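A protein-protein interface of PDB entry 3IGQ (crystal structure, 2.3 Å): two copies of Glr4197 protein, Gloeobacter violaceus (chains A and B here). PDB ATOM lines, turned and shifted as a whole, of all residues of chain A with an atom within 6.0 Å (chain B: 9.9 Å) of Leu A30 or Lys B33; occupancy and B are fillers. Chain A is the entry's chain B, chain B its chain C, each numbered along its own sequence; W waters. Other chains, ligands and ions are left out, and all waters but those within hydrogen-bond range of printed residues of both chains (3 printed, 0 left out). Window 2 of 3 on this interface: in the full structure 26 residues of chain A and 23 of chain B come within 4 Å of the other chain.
OE2 of Glu B35 is in hydrogen-bond range of OG1 of Thr A158 (3.5 Å).
The side-chain carboxylate (OE1) of Glu B35 lies within hydrogen-bond range of the backbone NH (N) of Ser A29 (2.6 Å).
The backbone NH (N) of Lys B33 is in hydrogen-bond range of the side-chain carboxylate (OD1) of Asp B31, at 3.1 Å.
OG1 of Thr B36 sits at hydrogen-bond distance from NH1 of Arg B109, at 2.7 Å.
O of Tyr A28 is in hydrogen-bond range of N of Lys A38 (2.8 Å).
The backbone NH of Ser B112 lies within hydrogen-bond range of the backbone carbonyl oxygen of Glu B35.
The side-chain carboxylate (OD1) of Asp B31 is in hydrogen-bond range of the backbone NH (N) of Glu B35 (2.9 Å).
The side-chain carboxylate (OD2) of Asp B31 is in hydrogen-bond range of the side-chain hydroxyl (OG1) of Thr B36 (2.7 Å).
Among the printed residues, merely in contact across the chains: Tyr A28 with Glu B35 (3.2 Å), Tyr A28 with Thr B36 (3.8 Å), Leu A30 with Lys B33 (3.4 Å), Leu A157 with Glu B35 (3.8 Å) and Thr A158 with Lys B33 (3.8 Å).
Lys B33 touches just these residues of chain A: Leu A30 (3.4 Å) and Thr A158 (3.8 Å).
Ser A29 touches just one residue of chain B: Glu B35 (2.6 Å).
Of the printed residues of chain A, Thr B36 touches Tyr A28 (3.8 Å).
Of the printed residues of chain B, Thr A158 touches Lys B33 and Glu B35.
Of the printed residues of chain B, Tyr A28 touches Glu B35 and Thr B36.
Of the printed residues of chain B, Leu A157 touches Glu B35.
Phe B37 touches none of the printed residues of chain A.
Lys A38 touches none of the printed residues of chain B.
The nearest printed residue of chain B that does not touch Thr A158 is Leu B114 (5.6 Å).
Among the printed residues, 7 pairs touch across the chains.
Among the printed residues, no Asp or Glu carboxylate lies within 4 Å of a Lys or Arg side-chain nitrogen of the other chain.
Ser A29 touches Glu B35, but with the chains exchanged Glu A35 does not touch Ser B29 (21.2 Å).
Of the 7 pairs that touch across the chains among the printed residues, none has its exchanged pair printed and touching as well.
Water W3 lies within hydrogen-bond range of OE1 of Glu B35, OD2 of Asp B31 and N of Ser A29.
Water W2 lies within hydrogen-bond range of NZ of Lys B33 (2.7 Å), O of Leu A30 (3.3 Å) and O of Asp A31 (3.4 Å).
Water W1 lies within hydrogen-bond range of the backbone carbonyl oxygen of Thr A158 (3.2 Å) and the side-chain amino group of Lys B33 (3.3 Å).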
ATOM      1  N   TYR A  28      30.316  15.677   7.916  1.00  0.00           N
ATOM      2  CA  TYR A  28      29.547  16.146   6.792  1.00  0.00           C
ATOM      3  C   TYR A  28      30.311  15.920   5.501  1.00  0.00           C
ATOM      4  O   TYR A  28      31.509  15.582   5.495  1.00  0.00           O
ATOM      5  CB  TYR A  28      29.175  17.647   6.945  1.00  0.00           C
ATOM      6  CG  TYR A  28      30.355  18.564   7.088  1.00  0.00           C
ATOM      7  CD1 TYR A  28      31.130  18.577   8.253  1.00  0.00           C
ATOM      8  CD2 TYR A  28      30.708  19.419   6.051  1.00  0.00           C
ATOM      9  CE1 TYR A  28      32.233  19.433   8.388  1.00  0.00           C
ATOM     10  CE2 TYR A  28      31.826  20.302   6.144  1.00  0.00           C
ATOM     11  CZ  TYR A  28      32.576  20.298   7.319  1.00  0.00           C
ATOM     12  OH  TYR A  28      33.694  21.128   7.421  1.00  0.00           O
ATOM     13  N   SER A  29      29.599  16.104   4.400  1.00  0.00           N
ATOM     14  CA  SER A  29      30.181  16.157   3.075  1.00  0.00           C
ATOM     15  C   SER A  29      30.893  14.866   2.701  1.00  0.00           C
ATOM     16  O   SER A  29      32.020  14.870   2.236  1.00  0.00           O
ATOM     17  CB  SER A  29      31.067  17.404   2.988  1.00  0.00           C
ATOM     18  OG  SER A  29      31.818  17.438   1.821  1.00  0.00           O
ATOM     19  N   LEU A  30      30.229  13.743   2.938  1.00  0.00           N
ATOM     20  CA  LEU A  30      30.652  12.486   2.387  1.00  0.00           C
ATOM     21  C   LEU A  30      30.781  12.641   0.868  1.00  0.00           C
ATOM     22  O   LEU A  30      29.878  13.161   0.253  1.00  0.00           O
ATOM     23  CB  LEU A  30      29.636  11.409   2.741  1.00  0.00           C
ATOM     24  CG  LEU A  30      29.956   9.951   2.381  1.00  0.00           C
ATOM     25  CD1 LEU A  30      31.157   9.450   3.263  1.00  0.00           C
ATOM     26  CD2 LEU A  30      28.716   9.092   2.561  1.00  0.00           C
ATOM     27  N   ASP A  31      31.904  12.225   0.266  1.00  0.00           N
ATOM     28  CA  ASP A  31      32.071  12.405  -1.173  1.00  0.00           C
ATOM     29  C   ASP A  31      31.290  11.372  -1.997  1.00  0.00           C
ATOM     30  O   ASP A  31      30.746  10.437  -1.438  1.00  0.00           O
ATOM     31  CB  ASP A  31      33.539  12.501  -1.587  1.00  0.00           C
ATOM     32  CG  ASP A  31      34.327  11.219  -1.347  1.00  0.00           C
ATOM     33  OD1 ASP A  31      33.796  10.085  -1.355  1.00  0.00           O
ATOM     34  OD2 ASP A  31      35.532  11.378  -1.170  1.00  0.00           O
ATOM     35  N   ASP A  32      31.203  11.562  -3.316  1.00  0.00           N
ATOM     36  CA  ASP A  32      30.375  10.678  -4.149  1.00  0.00           C
ATOM     37  C   ASP A  32      30.791   9.200  -4.102  1.00  0.00           C
ATOM     38  O   ASP A  32      30.001   8.345  -4.381  1.00  0.00           O
ATOM     39  CB  ASP A  32      30.421  11.130  -5.606  1.00  0.00           C
ATOM     40  CG  ASP A  32      29.766  12.478  -5.830  1.00  0.00           C
ATOM     41  OD1 ASP A  32      28.841  12.834  -5.073  1.00  0.00           O
ATOM     42  OD2 ASP A  32      30.174  13.168  -6.793  1.00  0.00           O
ATOM     43  N   ALA A  34      31.989   7.811  -1.322  1.00  0.00           N
ATOM     44  CA  ALA A  34      31.963   7.447   0.095  1.00  0.00           C
ATOM     45  C   ALA A  34      33.356   7.001   0.566  1.00  0.00           C
ATOM     46  O   ALA A  34      33.535   6.038   1.340  1.00  0.00           O
ATOM     47  CB  ALA A  34      30.900   6.412   0.365  1.00  0.00           C
ATOM     48  N   GLU A  35      34.352   7.746   0.115  1.00  0.00           N
ATOM     49  CA  GLU A  35      35.725   7.412   0.515  1.00  0.00           C
ATOM     50  C   GLU A  35      36.187   8.325   1.595  1.00  0.00           C
ATOM     51  O   GLU A  35      37.013   7.945   2.372  1.00  0.00           O
ATOM     52  CB  GLU A  35      36.702   7.516  -0.670  1.00  0.00           C
ATOM     53  CG  GLU A  35      36.484   6.426  -1.734  1.00  0.00           C
ATOM     54  CD  GLU A  35      37.219   6.694  -3.023  1.00  0.00           C
ATOM     55  OE1 GLU A  35      37.621   7.850  -3.335  1.00  0.00           O
ATOM     56  OE2 GLU A  35      37.397   5.728  -3.733  1.00  0.00           O
ATOM     57  N   THR A  36      35.688   9.551   1.572  1.00  0.00           N
ATOM     58  CA  THR A  36      36.167  10.612   2.450  1.00  0.00           C
ATOM     59  C   THR A  36      34.990  11.486   2.936  1.00  0.00           C
ATOM     60  O   THR A  36      33.901  11.521   2.317  1.00  0.00           O
ATOM     61  CB  THR A  36      37.244  11.534   1.775  1.00  0.00           C
ATOM     62  OG1 THR A  36      36.582  12.478   0.916  1.00  0.00           O
ATOM     63  CG2 THR A  36      38.249  10.742   0.996  1.00  0.00           C
ATOM     64  N   PHE A  37      35.201  12.148   4.065  1.00  0.00           N
ATOM     65  CA  PHE A  37      34.202  13.012   4.652  1.00  0.00           C
ATOM     66  C   PHE A  37      34.927  14.036   5.507  1.00  0.00           C
ATOM     67  O   PHE A  37      36.057  13.790   5.939  1.00  0.00           O
ATOM     68  CB  PHE A  37      33.224  12.208   5.496  1.00  0.00           C
ATOM     69  CG  PHE A  37      33.870  11.358   6.533  1.00  0.00           C
ATOM     70  CD1 PHE A  37      34.322  10.090   6.236  1.00  0.00           C
ATOM     71  CD2 PHE A  37      33.976  11.810   7.836  1.00  0.00           C
ATOM     72  CE1 PHE A  37      34.908   9.316   7.221  1.00  0.00           C
ATOM     73  CE2 PHE A  37      34.552  11.039   8.818  1.00  0.00           C
ATOM     74  CZ  PHE A  37      35.014   9.796   8.510  1.00  0.00           C
ATOM     75  N   LYS A  38      34.285  15.175   5.740  1.00  0.00           N
ATOM     76  CA  LYS A  38      34.844  16.180   6.621  1.00  0.00           C
ATOM     77  C   LYS A  38      34.416  16.015   8.082  1.00  0.00           C
ATOM     78  O   LYS A  38      33.332  15.521   8.416  1.00  0.00           O
ATOM     79  CB  LYS A  38      34.549  17.596   6.122  1.00  0.00           C
ATOM     80  CG  LYS A  38      35.310  17.933   4.827  1.00  0.00           C
ATOM     81  CD  LYS A  38      35.424  19.424   4.549  1.00  0.00           C
ATOM     82  CE  LYS A  38      36.494  20.046   5.442  1.00  0.00           C
ATOM     83  NZ  LYS A  38      36.796  21.444   5.018  1.00  0.00           N
ATOM     84  N   ARG A 109      39.575  16.548   6.224  1.00  0.00           N
ATOM     85  CA  ARG A 109      38.924  15.557   5.421  1.00  0.00           C
ATOM     86  C   ARG A 109      39.558  14.248   5.770  1.00  0.00           C
ATOM     87  O   ARG A 109      40.717  14.008   5.489  1.00  0.00           O
ATOM     88  CB  ARG A 109      39.041  15.887   3.920  1.00  0.00           C
ATOM     89  CG  ARG A 109      38.304  14.911   3.004  1.00  0.00           C
ATOM     90  CD  ARG A 109      38.084  15.481   1.585  1.00  0.00           C
ATOM     91  NE  ARG A 109      36.957  16.433   1.548  1.00  0.00           N
ATOM     92  CZ  ARG A 109      35.675  16.080   1.463  1.00  0.00           C
ATOM     93  NH1 ARG A 109      35.337  14.793   1.446  1.00  0.00           N
ATOM     94  NH2 ARG A 109      34.720  17.003   1.442  1.00  0.00           N
ATOM     95  N   LEU A 114      33.757   4.231   3.427  1.00  0.00           N
ATOM     96  CA  LEU A 114      32.640   3.393   3.848  1.00  0.00           C
ATOM     97  C   LEU A 114      32.579   2.122   2.978  1.00  0.00           C
ATOM     98  O   LEU A 114      32.803   2.170   1.773  1.00  0.00           O
ATOM     99  CB  LEU A 114      31.330   4.159   3.740  1.00  0.00           C
ATOM    100  CG  LEU A 114      30.977   5.053   4.916  1.00  0.00           C
ATOM    101  CD1 LEU A 114      31.930   6.232   5.085  1.00  0.00           C
ATOM    102  CD2 LEU A 114      29.570   5.509   4.754  1.00  0.00           C
ATOM    103  N   PHE A 156      25.781  10.401  12.314  1.00  0.00           N
ATOM    104  CA  PHE A 156      27.078  10.572  11.685  1.00  0.00           C
ATOM    105  C   PHE A 156      26.917  11.637  10.613  1.00  0.00           C
ATOM    106  O   PHE A 156      27.477  12.717  10.693  1.00  0.00           O
ATOM    107  CB  PHE A 156      27.597   9.245  11.099  1.00  0.00           C
ATOM    108  CG  PHE A 156      28.838   9.371  10.268  1.00  0.00           C
ATOM    109  CD1 PHE A 156      29.918  10.138  10.700  1.00  0.00           C
ATOM    110  CD2 PHE A 156      28.936   8.708   9.061  1.00  0.00           C
ATOM    111  CE1 PHE A 156      31.087  10.243   9.948  1.00  0.00           C
ATOM    112  CE2 PHE A 156      30.112   8.802   8.266  1.00  0.00           C
ATOM    113  CZ  PHE A 156      31.184   9.571   8.713  1.00  0.00           C
ATOM    114  N   LEU A 157      26.157  11.323   9.603  1.00  0.00           N
ATOM    115  CA  LEU A 157      25.784  12.291   8.628  1.00  0.00           C
ATOM    116  C   LEU A 157      24.612  11.646   7.956  1.00  0.00           C
ATOM    117  O   LEU A 157      24.143  10.600   8.396  1.00  0.00           O
ATOM    118  CB  LEU A 157      26.934  12.646   7.650  1.00  0.00           C
ATOM    119  CG  LEU A 157      27.554  11.590   6.730  1.00  0.00           C
ATOM    120  CD1 LEU A 157      26.691  11.355   5.513  1.00  0.00           C
ATOM    121  CD2 LEU A 157      28.910  12.043   6.333  1.00  0.00           C
ATOM    122  N   THR A 158      24.110  12.277   6.914  1.00  0.00           N
ATOM    123  CA  THR A 158      22.806  11.935   6.357  1.00  0.00           C
ATOM    124  C   THR A 158      22.784  10.494   5.930  1.00  0.00           C
ATOM    125  O   THR A 158      23.514  10.101   5.042  1.00  0.00           O
ATOM    126  CB  THR A 158      22.514  12.836   5.120  1.00  0.00           C
ATOM    127  OG1 THR A 158      22.488  14.241   5.512  1.00  0.00           O
ATOM    128  CG2 THR A 158      21.230  12.404   4.471  1.00  0.00           C
ATOM    129  N   TRP A 160      23.182   7.827   8.239  1.00  0.00           N
ATOM    130  CA  TRP A 160      23.994   6.980   9.106  1.00  0.00           C
ATOM    131  C   TRP A 160      23.953   7.463  10.549  1.00  0.00           C
ATOM    132  O   TRP A 160      24.145   8.646  10.830  1.00  0.00           O
ATOM    133  CB  TRP A 160      25.451   6.973   8.614  1.00  0.00           C
ATOM    134  CG  TRP A 160      25.626   6.393   7.239  1.00  0.00           C
ATOM    135  CD1 TRP A 160      25.581   7.063   6.039  1.00  0.00           C
ATOM    136  CD2 TRP A 160      25.941   5.032   6.920  1.00  0.00           C
ATOM    137  NE1 TRP A 160      25.830   6.186   4.987  1.00  0.00           N
ATOM    138  CE2 TRP A 160      26.050   4.939   5.506  1.00  0.00           C
ATOM    139  CE3 TRP A 160      26.158   3.881   7.690  1.00  0.00           C
ATOM    140  CZ2 TRP A 160      26.328   3.730   4.857  1.00  0.00           C
ATOM    141  CZ3 TRP A 160      26.425   2.679   7.036  1.00  0.00           C
ATOM    142  CH2 TRP A 160      26.499   2.614   5.642  1.00  0.00           C
ATOM    143  N   SER B  29      22.995  29.492  -0.159  1.00  0.00           N
ATOM    144  CA  SER B  29      23.889  28.419  -0.631  1.00  0.00           C
ATOM    145  C   SER B  29      23.864  27.198   0.264  1.00  0.00           C
ATOM    146  O   SER B  29      24.889  26.686   0.631  1.00  0.00           O
ATOM    147  CB  SER B  29      25.285  29.039  -0.796  1.00  0.00           C
ATOM    148  OG  SER B  29      26.276  28.108  -1.145  1.00  0.00           O
ATOM    149  N   LEU B  30      22.665  26.782   0.665  1.00  0.00           N
ATOM    150  CA  LEU B  30      22.474  25.461   1.270  1.00  0.00           C
ATOM    151  C   LEU B  30      23.102  24.411   0.320  1.00  0.00           C
ATOM    152  O   LEU B  30      22.814  24.454  -0.860  1.00  0.00           O
ATOM    153  CB  LEU B  30      20.999  25.177   1.487  1.00  0.00           C
ATOM    154  CG  LEU B  30      20.612  23.902   2.265  1.00  0.00           C
ATOM    155  CD1 LEU B  30      21.027  24.012   3.727  1.00  0.00           C
ATOM    156  CD2 LEU B  30      19.094  23.629   2.136  1.00  0.00           C
ATOM    157  N   ASP B  31      23.980  23.542   0.818  1.00  0.00           N
ATOM    158  CA  ASP B  31      24.614  22.488  -0.011  1.00  0.00           C
ATOM    159  C   ASP B  31      23.631  21.363  -0.379  1.00  0.00           C
ATOM    160  O   ASP B  31      22.538  21.339   0.129  1.00  0.00           O
ATOM    161  CB  ASP B  31      25.920  21.970   0.628  1.00  0.00           C
ATOM    162  CG  ASP B  31      25.705  21.172   1.895  1.00  0.00           C
ATOM    163  OD1 ASP B  31      24.636  20.539   2.083  1.00  0.00           O
ATOM    164  OD2 ASP B  31      26.624  21.180   2.712  1.00  0.00           O
ATOM    165  N   ASP B  32      24.006  20.480  -1.302  1.00  0.00           N
ATOM    166  CA  ASP B  32      23.148  19.391  -1.789  1.00  0.00           C
ATOM    167  C   ASP B  32      22.674  18.435  -0.700  1.00  0.00           C
ATOM    168  O   ASP B  32      21.631  17.836  -0.844  1.00  0.00           O
ATOM    169  CB  ASP B  32      23.910  18.544  -2.811  1.00  0.00           C
ATOM    170  CG  ASP B  32      24.168  19.264  -4.116  1.00  0.00           C
ATOM    171  OD1 ASP B  32      23.448  20.232  -4.450  1.00  0.00           O
ATOM    172  OD2 ASP B  32      25.088  18.830  -4.838  1.00  0.00           O
ATOM    173  N   LYS B  33      23.420  18.302   0.396  1.00  0.00           N
ATOM    174  CA  LYS B  33      22.996  17.413   1.458  1.00  0.00           C
ATOM    175  C   LYS B  33      22.264  18.129   2.563  1.00  0.00           C
ATOM    176  O   LYS B  33      21.858  17.498   3.573  1.00  0.00           O
ATOM    177  CB  LYS B  33      24.199  16.646   1.992  1.00  0.00           C
ATOM    178  CG  LYS B  33      24.659  15.479   1.060  1.00  0.00           C
ATOM    179  CD  LYS B  33      26.187  15.375   1.099  1.00  0.00           C
ATOM    180  CE  LYS B  33      26.751  14.512  -0.020  1.00  0.00           C
ATOM    181  NZ  LYS B  33      26.286  13.099   0.115  1.00  0.00           N
ATOM    182  N   ALA B  34      22.094  19.448   2.384  1.00  0.00           N
ATOM    183  CA  ALA B  34      21.437  20.301   3.393  1.00  0.00           C
ATOM    184  C   ALA B  34      22.156  20.154   4.750  1.00  0.00           C
ATOM    185  O   ALA B  34      21.526  20.030   5.831  1.00  0.00           O
ATOM    186  CB  ALA B  34      19.911  19.962   3.504  1.00  0.00           C
ATOM    187  N   GLU B  35      23.489  20.130   4.679  1.00  0.00           N
ATOM    188  CA  GLU B  35      24.265  19.959   5.898  1.00  0.00           C
ATOM    189  C   GLU B  35      24.836  21.284   6.315  1.00  0.00           C
ATOM    190  O   GLU B  35      25.048  21.508   7.492  1.00  0.00           O
ATOM    191  CB  GLU B  35      25.434  18.948   5.705  1.00  0.00           C
ATOM    192  CG  GLU B  35      24.985  17.512   5.659  1.00  0.00           C
ATOM    193  CD  GLU B  35      26.056  16.554   5.108  1.00  0.00           C
ATOM    194  OE1 GLU B  35      27.116  16.977   4.536  1.00  0.00           O
ATOM    195  OE2 GLU B  35      25.771  15.361   5.265  1.00  0.00           O
ATOM    196  N   THR B  36      25.137  22.129   5.339  1.00  0.00           N
ATOM    197  CA  THR B  36      25.850  23.354   5.598  1.00  0.00           C
ATOM    198  C   THR B  36      25.254  24.449   4.688  1.00  0.00           C
ATOM    199  O   THR B  36      24.609  24.163   3.643  1.00  0.00           O
ATOM    200  CB  THR B  36      27.369  23.237   5.356  1.00  0.00           C
ATOM    201  OG1 THR B  36      27.665  23.397   3.955  1.00  0.00           O
ATOM    202  CG2 THR B  36      27.921  21.939   5.850  1.00  0.00           C
ATOM    203  N   PHE B  37      25.438  25.698   5.108  1.00  0.00           N
ATOM    204  CA  PHE B  37      24.889  26.841   4.399  1.00  0.00           C
ATOM    205  C   PHE B  37      25.737  28.050   4.747  1.00  0.00           C
ATOM    206  O   PHE B  37      26.352  28.072   5.785  1.00  0.00           O
ATOM    207  CB  PHE B  37      23.410  27.061   4.785  1.00  0.00           C
ATOM    208  CG  PHE B  37      23.180  27.243   6.234  1.00  0.00           C
ATOM    209  CD1 PHE B  37      22.956  26.153   7.047  1.00  0.00           C
ATOM    210  CD2 PHE B  37      23.111  28.510   6.788  1.00  0.00           C
ATOM    211  CE1 PHE B  37      22.734  26.316   8.387  1.00  0.00           C
ATOM    212  CE2 PHE B  37      22.881  28.689   8.128  1.00  0.00           C
ATOM    213  CZ  PHE B  37      22.676  27.587   8.940  1.00  0.00           C
ATOM    214  N   ARG B 109      30.639  29.407   6.540  1.00  0.00           N
ATOM    215  CA  ARG B 109      29.783  28.298   6.187  1.00  0.00           C
ATOM    216  C   ARG B 109      29.496  27.590   7.516  1.00  0.00           C
ATOM    217  O   ARG B 109      30.385  27.059   8.142  1.00  0.00           O
ATOM    218  CB  ARG B 109      30.499  27.403   5.170  1.00  0.00           C
ATOM    219  CG  ARG B 109      29.719  26.141   4.777  1.00  0.00           C
ATOM    220  CD  ARG B 109      30.273  25.442   3.470  1.00  0.00           C
ATOM    221  NE  ARG B 109      29.908  26.160   2.238  1.00  0.00           N
ATOM    222  CZ  ARG B 109      28.669  26.173   1.700  1.00  0.00           C
ATOM    223  NH1 ARG B 109      27.636  25.486   2.244  1.00  0.00           N
ATOM    224  NH2 ARG B 109      28.440  26.891   0.607  1.00  0.00           N
ATOM    225  N   SER B 112      25.377  23.034  10.309  1.00  0.00           N
ATOM    226  CA  SER B 112      24.205  22.799  11.132  1.00  0.00           C
ATOM    227  C   SER B 112      23.162  22.150  10.183  1.00  0.00           C
ATOM    228  O   SER B 112      22.408  22.874   9.508  1.00  0.00           O
ATOM    229  CB  SER B 112      23.705  24.138  11.704  1.00  0.00           C
ATOM    230  OG  SER B 112      22.815  23.952  12.760  1.00  0.00           O
ATOM    231  N   PRO B 113      23.160  20.805  10.095  1.00  0.00           N
ATOM    232  CA  PRO B 113      22.325  20.072   9.142  1.00  0.00           C
ATOM    233  C   PRO B 113      20.828  20.270   9.308  1.00  0.00           C
ATOM    234  O   PRO B 113      20.334  20.271  10.419  1.00  0.00           O
ATOM    235  CB  PRO B 113      22.735  18.588   9.355  1.00  0.00           C
ATOM    236  CG  PRO B 113      24.099  18.675   9.905  1.00  0.00           C
ATOM    237  CD  PRO B 113      24.161  19.925  10.731  1.00  0.00           C
ATOM    238  N   LEU B 114      20.116  20.410   8.196  1.00  0.00           N
ATOM    239  CA  LEU B 114      18.664  20.264   8.180  1.00  0.00           C
ATOM    240  C   LEU B 114      18.342  18.780   8.266  1.00  0.00           C
ATOM    241  O   LEU B 114      18.890  17.982   7.532  1.00  0.00           O
ATOM    242  CB  LEU B 114      18.026  20.836   6.919  1.00  0.00           C
ATOM    243  CG  LEU B 114      18.047  22.315   6.557  1.00  0.00           C
ATOM    244  CD1 LEU B 114      19.416  22.858   6.685  1.00  0.00           C
ATOM    245  CD2 LEU B 114      17.492  22.628   5.230  1.00  0.00           C
ATOM    246  N   ASP B 115      17.472  18.429   9.191  1.00  0.00           N
ATOM    247  CA  ASP B 115      17.065  17.061   9.420  1.00  0.00           C
ATOM    248  C   ASP B 115      16.999  16.273   8.128  1.00  0.00           C
ATOM    249  O   ASP B 115      16.100  16.492   7.324  1.00  0.00           O
ATOM    250  CB  ASP B 115      15.685  17.075  10.053  1.00  0.00           C
ATOM    251  CG  ASP B 115      15.453  15.913  10.960  1.00  0.00           C
ATOM    252  OD1 ASP B 115      15.240  14.800  10.446  1.00  0.00           O
ATOM    253  OD2 ASP B 115      15.474  16.119  12.188  1.00  0.00           O
ATOM    254  N   GLN B 124      12.323  23.278  12.451  1.00  0.00           N
ATOM    255  CA  GLN B 124      13.624  22.944  13.045  1.00  0.00           C
ATOM    256  C   GLN B 124      14.541  24.093  13.491  1.00  0.00           C
ATOM    257  O   GLN B 124      14.345  25.252  13.120  1.00  0.00           O
ATOM    258  CB  GLN B 124      14.401  21.945  12.190  1.00  0.00           C
ATOM    259  CG  GLN B 124      14.392  22.168  10.734  1.00  0.00           C
ATOM    260  CD  GLN B 124      15.017  20.969  10.031  1.00  0.00           C
ATOM    261  OE1 GLN B 124      16.144  20.559  10.352  1.00  0.00           O
ATOM    262  NE2 GLN B 124      14.271  20.367   9.099  1.00  0.00           N
ATOM    263  N   TRP B 160      12.389  28.025   2.876  1.00  0.00           N
ATOM    264  CA  TRP B 160      12.310  28.013   4.331  1.00  0.00           C
ATOM    265  C   TRP B 160      12.139  29.391   4.918  1.00  0.00           C
ATOM    266  O   TRP B 160      12.891  30.329   4.606  1.00  0.00           O
ATOM    267  CB  TRP B 160      13.595  27.414   4.910  1.00  0.00           C
ATOM    268  CG  TRP B 160      13.843  26.000   4.533  1.00  0.00           C
ATOM    269  CD1 TRP B 160      14.493  25.532   3.407  1.00  0.00           C
ATOM    270  CD2 TRP B 160      13.477  24.852   5.282  1.00  0.00           C
ATOM    271  NE1 TRP B 160      14.536  24.165   3.409  1.00  0.00           N
ATOM    272  CE2 TRP B 160      13.918  23.714   4.547  1.00  0.00           C
ATOM    273  CE3 TRP B 160      12.812  24.659   6.505  1.00  0.00           C
ATOM    274  CZ2 TRP B 160      13.718  22.409   5.003  1.00  0.00           C
ATOM    275  CZ3 TRP B 160      12.604  23.349   6.949  1.00  0.00           C
ATOM    276  CH2 TRP B 160      13.049  22.251   6.205  1.00  0.00           C
ATOM    277  N   ARG B 192       9.410  24.996   6.807  1.00  0.00           N
ATOM    278  CA  ARG B 192       9.098  24.869   5.367  1.00  0.00           C
ATOM    279  C   ARG B 192       8.011  25.836   4.913  1.00  0.00           C
ATOM    280  O   ARG B 192       7.000  25.975   5.571  1.00  0.00           O
ATOM    281  CB  ARG B 192       8.680  23.433   5.019  1.00  0.00           C
ATOM    282  CG  ARG B 192       9.678  22.718   4.154  1.00  0.00           C
ATOM    283  CD  ARG B 192       9.375  21.221   3.986  1.00  0.00           C
ATOM    284  NE  ARG B 192      10.554  20.550   3.450  1.00  0.00           N
ATOM    285  CZ  ARG B 192      11.336  19.675   4.084  1.00  0.00           C
ATOM    286  NH1 ARG B 192      11.079  19.244   5.321  1.00  0.00           N
ATOM    287  NH2 ARG B 192      12.393  19.207   3.436  1.00  0.00           N
HETATM  288  O   HOH W   1      25.399  11.704   2.998  1.00  0.00           O
HETATM  289  O   HOH W   2      27.682  11.874  -1.829  1.00  0.00           O
HETATM  290  O   HOH W   3      28.063  18.752   2.845  1.00  0.00           O
